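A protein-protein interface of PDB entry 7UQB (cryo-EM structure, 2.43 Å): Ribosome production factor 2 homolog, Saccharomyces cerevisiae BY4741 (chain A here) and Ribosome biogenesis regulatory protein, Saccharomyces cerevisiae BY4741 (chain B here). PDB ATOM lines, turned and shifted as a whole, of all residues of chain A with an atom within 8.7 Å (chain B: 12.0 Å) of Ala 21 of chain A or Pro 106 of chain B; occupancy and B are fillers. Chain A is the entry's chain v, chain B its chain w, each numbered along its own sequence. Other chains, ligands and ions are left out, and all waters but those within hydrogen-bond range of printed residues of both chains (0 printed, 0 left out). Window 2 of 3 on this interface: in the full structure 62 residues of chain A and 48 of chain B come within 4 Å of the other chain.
NH1 of Arg 101 of chain B lies within hydrogen-bond range of O of Lys 22 of chain A, at 3.0 Å. The backbone carbonyl oxygen (O) of Leu 23 of chain A sits at hydrogen-bond distance from the guanidinium group (NH1) of Arg 101 of chain B, at 3.3 Å. OE2 of Glu 25 of chain A is in salt-bridge range of NH2 of Arg 101 of chain B, at 3.5 Å. OD1 of Asp 83 of chain A is in salt-bridge range of NZ of Lys 103 of chain B (3.7 Å). The backbone NH of Gly 107 of chain A sits at hydrogen-bond distance from the backbone carbonyl oxygen of Glu 102 of chain B, at 2.6 Å. The side-chain carboxylate (OE2) of Glu 102 of chain B lies close to the side-chain carboxylate (OE1) of Glu 25 of chain A, 3.0 Å away. The side-chain carboxylate (OE2) of Glu 102 of chain B lies close to the backbone carbonyl oxygen (O) of Asn 26 of chain A (3.5 Å).
The guanidinium group (NE) of Arg 19 of chain A is in salt-bridge range of the side-chain carboxylate (OD2) of Asp 83 of chain A. OE2 of Glu 25 of chain A sits at hydrogen-bond distance from N of Lys 22 of chain A (2.9 Å). The guanidinium group (NH2) of Arg 101 of chain B is in hydrogen-bond range of the backbone carbonyl oxygen (O) of Lys 103 of chain B (2.7 Å). NH2 of Arg 101 of chain B is in hydrogen-bond range of O of Pro 104 of chain B. NZ of Lys 103 of chain B lies within salt-bridge range of OE1 of Glu 102 of chain B (2.6 Å).
Among the printed residues, pairs that only touch across the chains: Arg 19 of chain A with Lys 103 of chain B, Ala 21 of chain A with Lys 103 of chain B, Ala 21 of chain A with Pro 104 of chain B, Ala 21 of chain A with Pro 106 of chain B, Lys 22 of chain A with Pro 106 of chain B, Leu 23 of chain A with Pro 106 of chain B, Glu 25 of chain A with Lys 103 of chain B, Phe 106 of chain A with Arg 101 of chain B, Phe 106 of chain A with Glu 102 of chain B, Phe 106 of chain A with Lys 103 of chain B, Phe 106 of chain A with Pro 104 of chain B, Gly 107 of chain A with Pro 104 of chain B, Lys 251 of chain A with Leu 105 of chain B and Pro 252 of chain A with Leu 105 of chain B.
Ala 21 of chain A touches three residues of chain B. Of chain B, only Arg 101 and Pro 106 come within 4 Å of Lys 22 of chain A. Leu 23 of chain A touches two residues of chain B. Of the printed residues of chain B, Phe 106 of chain A touches Arg 101, Glu 102, Lys 103 and Pro 104. Tyr 108 of chain A touches none of the printed residues of chain B. Pro 252 of chain A touches one residue of chain B. Of the printed residues of chain A, Arg 101 of chain B touches Lys 22 (3.0 Å), Leu 23 (3.3 Å), Glu 25 (3.5 Å) and Phe 106 (3.2 Å). Of the printed residues of chain A, Glu 102 of chain B touches Glu 25 (3.0 Å), Asn 26 (3.5 Å), Phe 106 (3.3 Å) and Gly 107 (2.6 Å). Pro 106 of chain B touches just these residues of chain A: Ala 21 (3.9 Å), Lys 22 (3.8 Å) and Leu 23 (3.9 Å). Ala 108 of chain B touches none of the printed residues of chain A. The nearest residue of chain B that does not touch Ala 21 of chain A is Arg 101 of chain B (4.7 Å). The nearest residue of chain A that does not touch Pro 106 of chain B is Gln 254 of chain A (6.0 Å).
Hydrophobic or aromatic side chains of chain B within 4 Å of the printed part of chain A: Pro 104, Leu 105 and Pro 106. Hydrophobic or aromatic side chains of chain A within 4 Å of the printed part of chain B: Ala 21, Leu 23, Phe 106 and Pro 252. Among the printed residues, Asp or Glu carboxylates within 4 Å of a Lys or Arg side-chain nitrogen of the other chain: Glu 25 of chain A with Arg 101 of chain B (3.5 Å) and Asp 83 of chain A with Lys 103 of chain B (3.7 Å).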
ATOM      1  N   LEU A  16     -20.158  16.389  28.998  1.00  0.00           N
ATOM      2  CA  LEU A  16     -19.890  17.646  28.301  1.00  0.00           C
ATOM      3  C   LEU A  16     -18.918  18.522  29.087  1.00  0.00           C
ATOM      4  O   LEU A  16     -18.036  19.162  28.502  1.00  0.00           O
ATOM      5  CB  LEU A  16     -21.196  18.398  28.046  1.00  0.00           C
ATOM      6  CG  LEU A  16     -22.179  17.742  27.077  1.00  0.00           C
ATOM      7  CD1 LEU A  16     -23.427  18.595  26.916  1.00  0.00           C
ATOM      8  CD2 LEU A  16     -21.516  17.487  25.733  1.00  0.00           C
ATOM      9  N   VAL A  17     -19.077  18.575  30.411  1.00  0.00           N
ATOM     10  CA  VAL A  17     -18.167  19.356  31.247  1.00  0.00           C
ATOM     11  C   VAL A  17     -16.761  18.766  31.207  1.00  0.00           C
ATOM     12  O   VAL A  17     -15.768  19.498  31.133  1.00  0.00           O
ATOM     13  CB  VAL A  17     -18.712  19.445  32.685  1.00  0.00           C
ATOM     14  CG1 VAL A  17     -17.671  20.026  33.623  1.00  0.00           C
ATOM     15  CG2 VAL A  17     -19.972  20.292  32.715  1.00  0.00           C
ATOM     16  N   LYS A  18     -16.654  17.435  31.251  1.00  0.00           N
ATOM     17  CA  LYS A  18     -15.354  16.787  31.118  1.00  0.00           C
ATOM     18  C   LYS A  18     -14.718  17.085  29.766  1.00  0.00           C
ATOM     19  O   LYS A  18     -13.492  17.206  29.665  1.00  0.00           O
ATOM     20  CB  LYS A  18     -15.511  15.278  31.317  1.00  0.00           C
ATOM     21  CG  LYS A  18     -14.215  14.489  31.312  1.00  0.00           C
ATOM     22  CD  LYS A  18     -14.491  12.998  31.424  1.00  0.00           C
ATOM     23  CE  LYS A  18     -15.266  12.670  32.693  1.00  0.00           C
ATOM     24  NZ  LYS A  18     -15.612  11.224  32.783  1.00  0.00           N
ATOM     25  N   ARG A  19     -15.537  17.219  28.724  1.00  0.00           N
ATOM     26  CA  ARG A  19     -15.030  17.504  27.387  1.00  0.00           C
ATOM     27  C   ARG A  19     -14.612  18.964  27.215  1.00  0.00           C
ATOM     28  O   ARG A  19     -13.661  19.244  26.478  1.00  0.00           O
ATOM     29  CB  ARG A  19     -16.096  17.125  26.359  1.00  0.00           C
ATOM     30  CG  ARG A  19     -15.680  17.279  24.915  1.00  0.00           C
ATOM     31  CD  ARG A  19     -16.526  16.398  24.016  1.00  0.00           C
ATOM     32  NE  ARG A  19     -16.353  14.986  24.338  1.00  0.00           N
ATOM     33  CZ  ARG A  19     -16.863  13.987  23.631  1.00  0.00           C
ATOM     34  NH1 ARG A  19     -17.603  14.207  22.556  1.00  0.00           N
ATOM     35  NH2 ARG A  19     -16.623  12.736  24.011  1.00  0.00           N
ATOM     36  N   GLU A  20     -15.292  19.892  27.886  1.00  0.00           N
ATOM     37  CA  GLU A  20     -15.041  21.315  27.682  1.00  0.00           C
ATOM     38  C   GLU A  20     -13.652  21.714  28.184  1.00  0.00           C
ATOM     39  O   GLU A  20     -13.018  21.013  28.977  1.00  0.00           O
ATOM     40  CB  GLU A  20     -16.107  22.159  28.384  1.00  0.00           C
ATOM     41  CG  GLU A  20     -15.826  22.424  29.855  1.00  0.00           C
ATOM     42  CD  GLU A  20     -16.975  23.117  30.561  1.00  0.00           C
ATOM     43  OE1 GLU A  20     -18.017  23.358  29.916  1.00  0.00           O
ATOM     44  OE2 GLU A  20     -16.838  23.417  31.765  1.00  0.00           O
ATOM     45  N   ALA A  21     -13.184  22.864  27.701  1.00  0.00           N
ATOM     46  CA  ALA A  21     -11.845  23.343  28.010  1.00  0.00           C
ATOM     47  C   ALA A  21     -11.756  23.836  29.453  1.00  0.00           C
ATOM     48  O   ALA A  21     -12.756  24.175  30.089  1.00  0.00           O
ATOM     49  CB  ALA A  21     -11.442  24.462  27.051  1.00  0.00           C
ATOM     50  N   LYS A  22     -10.526  23.882  29.964  1.00  0.00           N
ATOM     51  CA  LYS A  22     -10.288  24.230  31.357  1.00  0.00           C
ATOM     52  C   LYS A  22      -8.883  24.789  31.516  1.00  0.00           C
ATOM     53  O   LYS A  22      -8.029  24.637  30.639  1.00  0.00           O
ATOM     54  CB  LYS A  22     -10.492  23.017  32.270  1.00  0.00           C
ATOM     55  CG  LYS A  22      -9.800  21.764  31.775  1.00  0.00           C
ATOM     56  CD  LYS A  22     -10.359  20.528  32.449  1.00  0.00           C
ATOM     57  CE  LYS A  22     -11.845  20.387  32.178  1.00  0.00           C
ATOM     58  NZ  LYS A  22     -12.416  19.187  32.843  1.00  0.00           N
ATOM     59  N   LEU A  23      -8.658  25.453  32.656  1.00  0.00           N
ATOM     60  CA  LEU A  23      -7.353  26.048  32.934  1.00  0.00           C
ATOM     61  C   LEU A  23      -6.271  24.985  33.077  1.00  0.00           C
ATOM     62  O   LEU A  23      -5.177  25.126  32.519  1.00  0.00           O
ATOM     63  CB  LEU A  23      -7.425  26.902  34.199  1.00  0.00           C
ATOM     64  CG  LEU A  23      -8.462  28.025  34.234  1.00  0.00           C
ATOM     65  CD1 LEU A  23      -8.351  28.804  35.535  1.00  0.00           C
ATOM     66  CD2 LEU A  23      -8.304  28.946  33.036  1.00  0.00           C
ATOM     67  N   VAL A  24      -6.555  23.920  33.817  1.00  0.00           N
ATOM     68  CA  VAL A  24      -5.631  22.807  33.998  1.00  0.00           C
ATOM     69  C   VAL A  24      -6.201  21.629  33.223  1.00  0.00           C
ATOM     70  O   VAL A  24      -7.200  21.026  33.637  1.00  0.00           O
ATOM     71  CB  VAL A  24      -5.431  22.459  35.479  1.00  0.00           C
ATOM     72  CG1 VAL A  24      -4.271  21.491  35.644  1.00  0.00           C
ATOM     73  CG2 VAL A  24      -5.204  23.722  36.292  1.00  0.00           C
ATOM     74  N   GLU A  25      -5.576  21.302  32.099  1.00  0.00           N
ATOM     75  CA  GLU A  25      -6.119  20.294  31.203  1.00  0.00           C
ATOM     76  C   GLU A  25      -5.862  18.886  31.723  1.00  0.00           C
ATOM     77  O   GLU A  25      -4.867  18.618  32.402  1.00  0.00           O
ATOM     78  CB  GLU A  25      -5.529  20.448  29.802  1.00  0.00           C
ATOM     79  CG  GLU A  25      -6.134  21.593  29.012  1.00  0.00           C
ATOM     80  CD  GLU A  25      -7.629  21.428  28.796  1.00  0.00           C
ATOM     81  OE1 GLU A  25      -8.095  20.277  28.656  1.00  0.00           O
ATOM     82  OE2 GLU A  25      -8.340  22.454  28.771  1.00  0.00           O
ATOM     83  N   ASN A  26      -6.781  17.983  31.391  1.00  0.00           N
ATOM     84  CA  ASN A  26      -6.633  16.579  31.733  1.00  0.00           C
ATOM     85  C   ASN A  26      -5.576  15.931  30.839  1.00  0.00           C
ATOM     86  O   ASN A  26      -4.982  16.565  29.962  1.00  0.00           O
ATOM     87  CB  ASN A  26      -7.972  15.856  31.599  1.00  0.00           C
ATOM     88  CG  ASN A  26      -9.075  16.506  32.418  1.00  0.00           C
ATOM     89  OD1 ASN A  26      -8.812  17.196  33.401  1.00  0.00           O
ATOM     90  ND2 ASN A  26     -10.319  16.282  32.014  1.00  0.00           N
ATOM     91  N   ASP A  83     -13.090  12.886  21.550  1.00  0.00           N
ATOM     92  CA  ASP A  83     -12.439  13.806  22.489  1.00  0.00           C
ATOM     93  C   ASP A  83     -10.961  13.461  22.669  1.00  0.00           C
ATOM     94  O   ASP A  83     -10.403  13.571  23.762  1.00  0.00           O
ATOM     95  CB  ASP A  83     -13.164  13.835  23.839  1.00  0.00           C
ATOM     96  CG  ASP A  83     -12.872  15.095  24.633  1.00  0.00           C
ATOM     97  OD1 ASP A  83     -12.416  16.087  24.030  1.00  0.00           O
ATOM     98  OD2 ASP A  83     -13.088  15.089  25.863  1.00  0.00           O
ATOM     99  N   PHE A 106      -5.358  20.677  18.029  1.00  0.00           N
ATOM    100  CA  PHE A 106      -5.609  21.775  18.955  1.00  0.00           C
ATOM    101  C   PHE A 106      -7.023  22.281  18.727  1.00  0.00           C
ATOM    102  O   PHE A 106      -7.329  22.802  17.650  1.00  0.00           O
ATOM    103  CB  PHE A 106      -4.597  22.910  18.766  1.00  0.00           C
ATOM    104  CG  PHE A 106      -4.959  24.171  19.503  1.00  0.00           C
ATOM    105  CD1 PHE A 106      -4.718  24.289  20.860  1.00  0.00           C
ATOM    106  CD2 PHE A 106      -5.537  25.241  18.834  1.00  0.00           C
ATOM    107  CE1 PHE A 106      -5.050  25.445  21.541  1.00  0.00           C
ATOM    108  CE2 PHE A 106      -5.875  26.397  19.510  1.00  0.00           C
ATOM    109  CZ  PHE A 106      -5.628  26.500  20.866  1.00  0.00           C
ATOM    110  N   GLY A 107      -7.872  22.141  19.740  1.00  0.00           N
ATOM    111  CA  GLY A 107      -9.253  22.586  19.622  1.00  0.00           C
ATOM    112  C   GLY A 107     -10.024  21.879  18.531  1.00  0.00           C
ATOM    113  O   GLY A 107     -10.776  22.523  17.788  1.00  0.00           O
ATOM    114  N   TYR A 108      -9.827  20.565  18.399  1.00  0.00           N
ATOM    115  CA  TYR A 108     -10.485  19.713  17.407  1.00  0.00           C
ATOM    116  C   TYR A 108     -10.141  20.109  15.974  1.00  0.00           C
ATOM    117  O   TYR A 108     -10.868  19.761  15.040  1.00  0.00           O
ATOM    118  CB  TYR A 108     -12.004  19.687  17.612  1.00  0.00           C
ATOM    119  CG  TYR A 108     -12.409  19.123  18.952  1.00  0.00           C
ATOM    120  CD1 TYR A 108     -11.626  18.166  19.584  1.00  0.00           C
ATOM    121  CD2 TYR A 108     -13.563  19.553  19.592  1.00  0.00           C
ATOM    122  CE1 TYR A 108     -11.980  17.649  20.806  1.00  0.00           C
ATOM    123  CE2 TYR A 108     -13.930  19.036  20.819  1.00  0.00           C
ATOM    124  CZ  TYR A 108     -13.130  18.084  21.420  1.00  0.00           C
ATOM    125  OH  TYR A 108     -13.478  17.562  22.641  1.00  0.00           O
ATOM    126  N   LYS A 251      -0.811  30.893  28.144  1.00  0.00           N
ATOM    127  CA  LYS A 251      -0.908  30.411  29.513  1.00  0.00           C
ATOM    128  C   LYS A 251      -2.100  31.051  30.221  1.00  0.00           C
ATOM    129  O   LYS A 251      -2.450  32.200  29.937  1.00  0.00           O
ATOM    130  CB  LYS A 251       0.377  30.718  30.291  1.00  0.00           C
ATOM    131  CG  LYS A 251       1.651  30.283  29.581  1.00  0.00           C
ATOM    132  CD  LYS A 251       1.734  28.771  29.447  1.00  0.00           C
ATOM    133  CE  LYS A 251       2.919  28.359  28.584  1.00  0.00           C
ATOM    134  NZ  LYS A 251       4.201  28.930  29.081  1.00  0.00           N
ATOM    135  N   PRO A 252      -2.746  30.331  31.146  1.00  0.00           N
ATOM    136  CA  PRO A 252      -3.963  30.884  31.767  1.00  0.00           C
ATOM    137  C   PRO A 252      -3.692  32.003  32.758  1.00  0.00           C
ATOM    138  O   PRO A 252      -4.451  32.978  32.791  1.00  0.00           O
ATOM    139  CB  PRO A 252      -4.594  29.660  32.443  1.00  0.00           C
ATOM    140  CG  PRO A 252      -3.442  28.754  32.718  1.00  0.00           C
ATOM    141  CD  PRO A 252      -2.476  28.951  31.587  1.00  0.00           C
ATOM    142  N   GLN A 254      -4.395  32.595  35.593  1.00  0.00           N
ATOM    143  CA  GLN A 254      -5.351  32.743  36.686  1.00  0.00           C
ATOM    144  C   GLN A 254      -4.864  32.034  37.940  1.00  0.00           C
ATOM    145  O   GLN A 254      -5.252  32.404  39.053  1.00  0.00           O
ATOM    146  CB  GLN A 254      -6.715  32.187  36.275  1.00  0.00           C
ATOM    147  CG  GLN A 254      -7.051  32.348  34.801  1.00  0.00           C
ATOM    148  CD  GLN A 254      -7.597  33.719  34.470  1.00  0.00           C
ATOM    149  OE1 GLN A 254      -7.842  34.534  35.360  1.00  0.00           O
ATOM    150  NE2 GLN A 254      -7.795  33.983  33.185  1.00  0.00           N
ATOM    151  N   PRO B 100       2.224  22.282  23.521  1.00  0.00           N
ATOM    152  CA  PRO B 100       0.949  22.922  23.185  1.00  0.00           C
ATOM    153  C   PRO B 100      -0.218  22.271  23.913  1.00  0.00           C
ATOM    154  O   PRO B 100      -0.207  21.075  24.211  1.00  0.00           O
ATOM    155  CB  PRO B 100       0.842  22.722  21.669  1.00  0.00           C
ATOM    156  CG  PRO B 100       1.655  21.513  21.394  1.00  0.00           C
ATOM    157  CD  PRO B 100       2.790  21.541  22.381  1.00  0.00           C
ATOM    158  N   ARG B 101      -1.233  23.081  24.195  1.00  0.00           N
ATOM    159  CA  ARG B 101      -2.438  22.588  24.839  1.00  0.00           C
ATOM    160  C   ARG B 101      -3.339  21.887  23.828  1.00  0.00           C
ATOM    161  O   ARG B 101      -3.242  22.098  22.616  1.00  0.00           O
ATOM    162  CB  ARG B 101      -3.209  23.729  25.501  1.00  0.00           C
ATOM    163  CG  ARG B 101      -2.363  24.668  26.335  1.00  0.00           C
ATOM    164  CD  ARG B 101      -3.189  25.270  27.453  1.00  0.00           C
ATOM    165  NE  ARG B 101      -4.599  25.357  27.095  1.00  0.00           N
ATOM    166  CZ  ARG B 101      -5.592  25.322  27.971  1.00  0.00           C
ATOM    167  NH1 ARG B 101      -5.365  25.199  29.267  1.00  0.00           N
ATOM    168  NH2 ARG B 101      -6.845  25.403  27.536  1.00  0.00           N
ATOM    169  N   GLU B 102      -4.228  21.039  24.345  1.00  0.00           N
ATOM    170  CA  GLU B 102      -5.193  20.368  23.484  1.00  0.00           C
ATOM    171  C   GLU B 102      -6.332  21.290  23.067  1.00  0.00           C
ATOM    172  O   GLU B 102      -6.852  21.160  21.954  1.00  0.00           O
ATOM    173  CB  GLU B 102      -5.752  19.128  24.183  1.00  0.00           C
ATOM    174  CG  GLU B 102      -6.190  19.353  25.619  1.00  0.00           C
ATOM    175  CD  GLU B 102      -7.008  18.198  26.162  1.00  0.00           C
ATOM    176  OE1 GLU B 102      -7.776  17.596  25.381  1.00  0.00           O
ATOM    177  OE2 GLU B 102      -6.881  17.886  27.365  1.00  0.00           O
ATOM    178  N   LYS B 103      -6.729  22.217  23.932  1.00  0.00           N
ATOM    179  CA  LYS B 103      -7.834  23.125  23.671  1.00  0.00           C
ATOM    180  C   LYS B 103      -7.439  24.535  24.079  1.00  0.00           C
ATOM    181  O   LYS B 103      -6.589  24.712  24.961  1.00  0.00           O
ATOM    182  CB  LYS B 103      -9.100  22.696  24.430  1.00  0.00           C
ATOM    183  CG  LYS B 103      -9.891  21.598  23.739  1.00  0.00           C
ATOM    184  CD  LYS B 103     -10.962  21.029  24.650  1.00  0.00           C
ATOM    185  CE  LYS B 103     -10.383  19.994  25.599  1.00  0.00           C
ATOM    186  NZ  LYS B 103      -9.993  18.754  24.875  1.00  0.00           N
ATOM    187  N   PRO B 104      -8.024  25.554  23.452  1.00  0.00           N
ATOM    188  CA  PRO B 104      -7.729  26.935  23.847  1.00  0.00           C
ATOM    189  C   PRO B 104      -8.264  27.253  25.236  1.00  0.00           C
ATOM    190  O   PRO B 104      -9.058  26.517  25.822  1.00  0.00           O
ATOM    191  CB  PRO B 104      -8.427  27.776  22.773  1.00  0.00           C
ATOM    192  CG  PRO B 104      -9.439  26.868  22.167  1.00  0.00           C
ATOM    193  CD  PRO B 104      -8.843  25.499  22.230  1.00  0.00           C
ATOM    194  N   LEU B 105      -7.794  28.383  25.761  1.00  0.00           N
ATOM    195  CA  LEU B 105      -8.187  28.822  27.089  1.00  0.00           C
ATOM    196  C   LEU B 105      -9.676  29.165  27.128  1.00  0.00           C
ATOM    197  O   LEU B 105     -10.243  29.625  26.134  1.00  0.00           O
ATOM    198  CB  LEU B 105      -7.367  30.037  27.511  1.00  0.00           C
ATOM    199  CG  LEU B 105      -5.909  29.770  27.882  1.00  0.00           C
ATOM    200  CD1 LEU B 105      -5.208  31.066  28.254  1.00  0.00           C
ATOM    201  CD2 LEU B 105      -5.828  28.763  29.015  1.00  0.00           C
ATOM    202  N   PRO B 106     -10.335  28.935  28.268  1.00  0.00           N
ATOM    203  CA  PRO B 106     -11.758  29.287  28.379  1.00  0.00           C
ATOM    204  C   PRO B 106     -11.973  30.791  28.349  1.00  0.00           C
ATOM    205  O   PRO B 106     -11.561  31.502  29.271  1.00  0.00           O
ATOM    206  CB  PRO B 106     -12.168  28.688  29.732  1.00  0.00           C
ATOM    207  CG  PRO B 106     -11.093  27.698  30.070  1.00  0.00           C
ATOM    208  CD  PRO B 106      -9.842  28.250  29.474  1.00  0.00           C
ATOM    209  N   LYS B 107     -12.605  31.283  27.287  1.00  0.00           N
ATOM    210  CA  LYS B 107     -12.905  32.704  27.185  1.00  0.00           C
ATOM    211  C   LYS B 107     -13.925  33.109  28.240  1.00  0.00           C
ATOM    212  O   LYS B 107     -14.879  32.378  28.518  1.00  0.00           O
ATOM    213  CB  LYS B 107     -13.434  33.038  25.789  1.00  0.00           C
ATOM    214  CG  LYS B 107     -12.351  33.263  24.745  1.00  0.00           C
ATOM    215  CD  LYS B 107     -12.939  33.331  23.340  1.00  0.00           C
ATOM    216  CE  LYS B 107     -14.083  34.333  23.249  1.00  0.00           C
ATOM    217  NZ  LYS B 107     -13.646  35.730  23.519  1.00  0.00           N
ATOM    218  N   ALA B 108     -13.711  34.277  28.838  1.00  0.00           N
ATOM    219  CA  ALA B 108     -14.664  34.799  29.806  1.00  0.00           C
ATOM    220  C   ALA B 108     -15.921  35.265  29.086  1.00  0.00           C
ATOM    221  O   ALA B 108     -15.845  35.984  28.084  1.00  0.00           O
ATOM    222  CB  ALA B 108     -14.045  35.947  30.600  1.00  0.00           C
ATOM    223  N   LYS B 109     -17.077  34.841  29.588  1.00  0.00           N
ATOM    224  CA  LYS B 109     -18.342  35.215  28.975  1.00  0.00           C
ATOM    225  C   LYS B 109     -18.566  36.716  29.101  1.00  0.00           C
ATOM    226  O   LYS B 109     -18.310  37.312  30.150  1.00  0.00           O
ATOM    227  CB  LYS B 109     -19.495  34.450  29.625  1.00  0.00           C
ATOM    228  CG  LYS B 109     -20.854  34.716  29.000  1.00  0.00           C
ATOM    229  CD  LYS B 109     -20.882  34.299  27.536  1.00  0.00           C
ATOM    230  CE  LYS B 109     -20.649  32.806  27.387  1.00  0.00           C
ATOM    231  NZ  LYS B 109     -20.622  32.389  25.960  1.00  0.00           N
ATOM    232  N   ALA B 110     -19.036  37.327  28.015  1.00  0.00           N
ATOM    233  CA  ALA B 110     -19.303  38.756  28.019  1.00  0.00           C
ATOM    234  C   ALA B 110     -20.427  39.082  28.994  1.00  0.00           C
ATOM    235  O   ALA B 110     -21.270  38.238  29.309  1.00  0.00           O
ATOM    236  CB  ALA B 110     -19.665  39.238  26.614  1.00  0.00           C
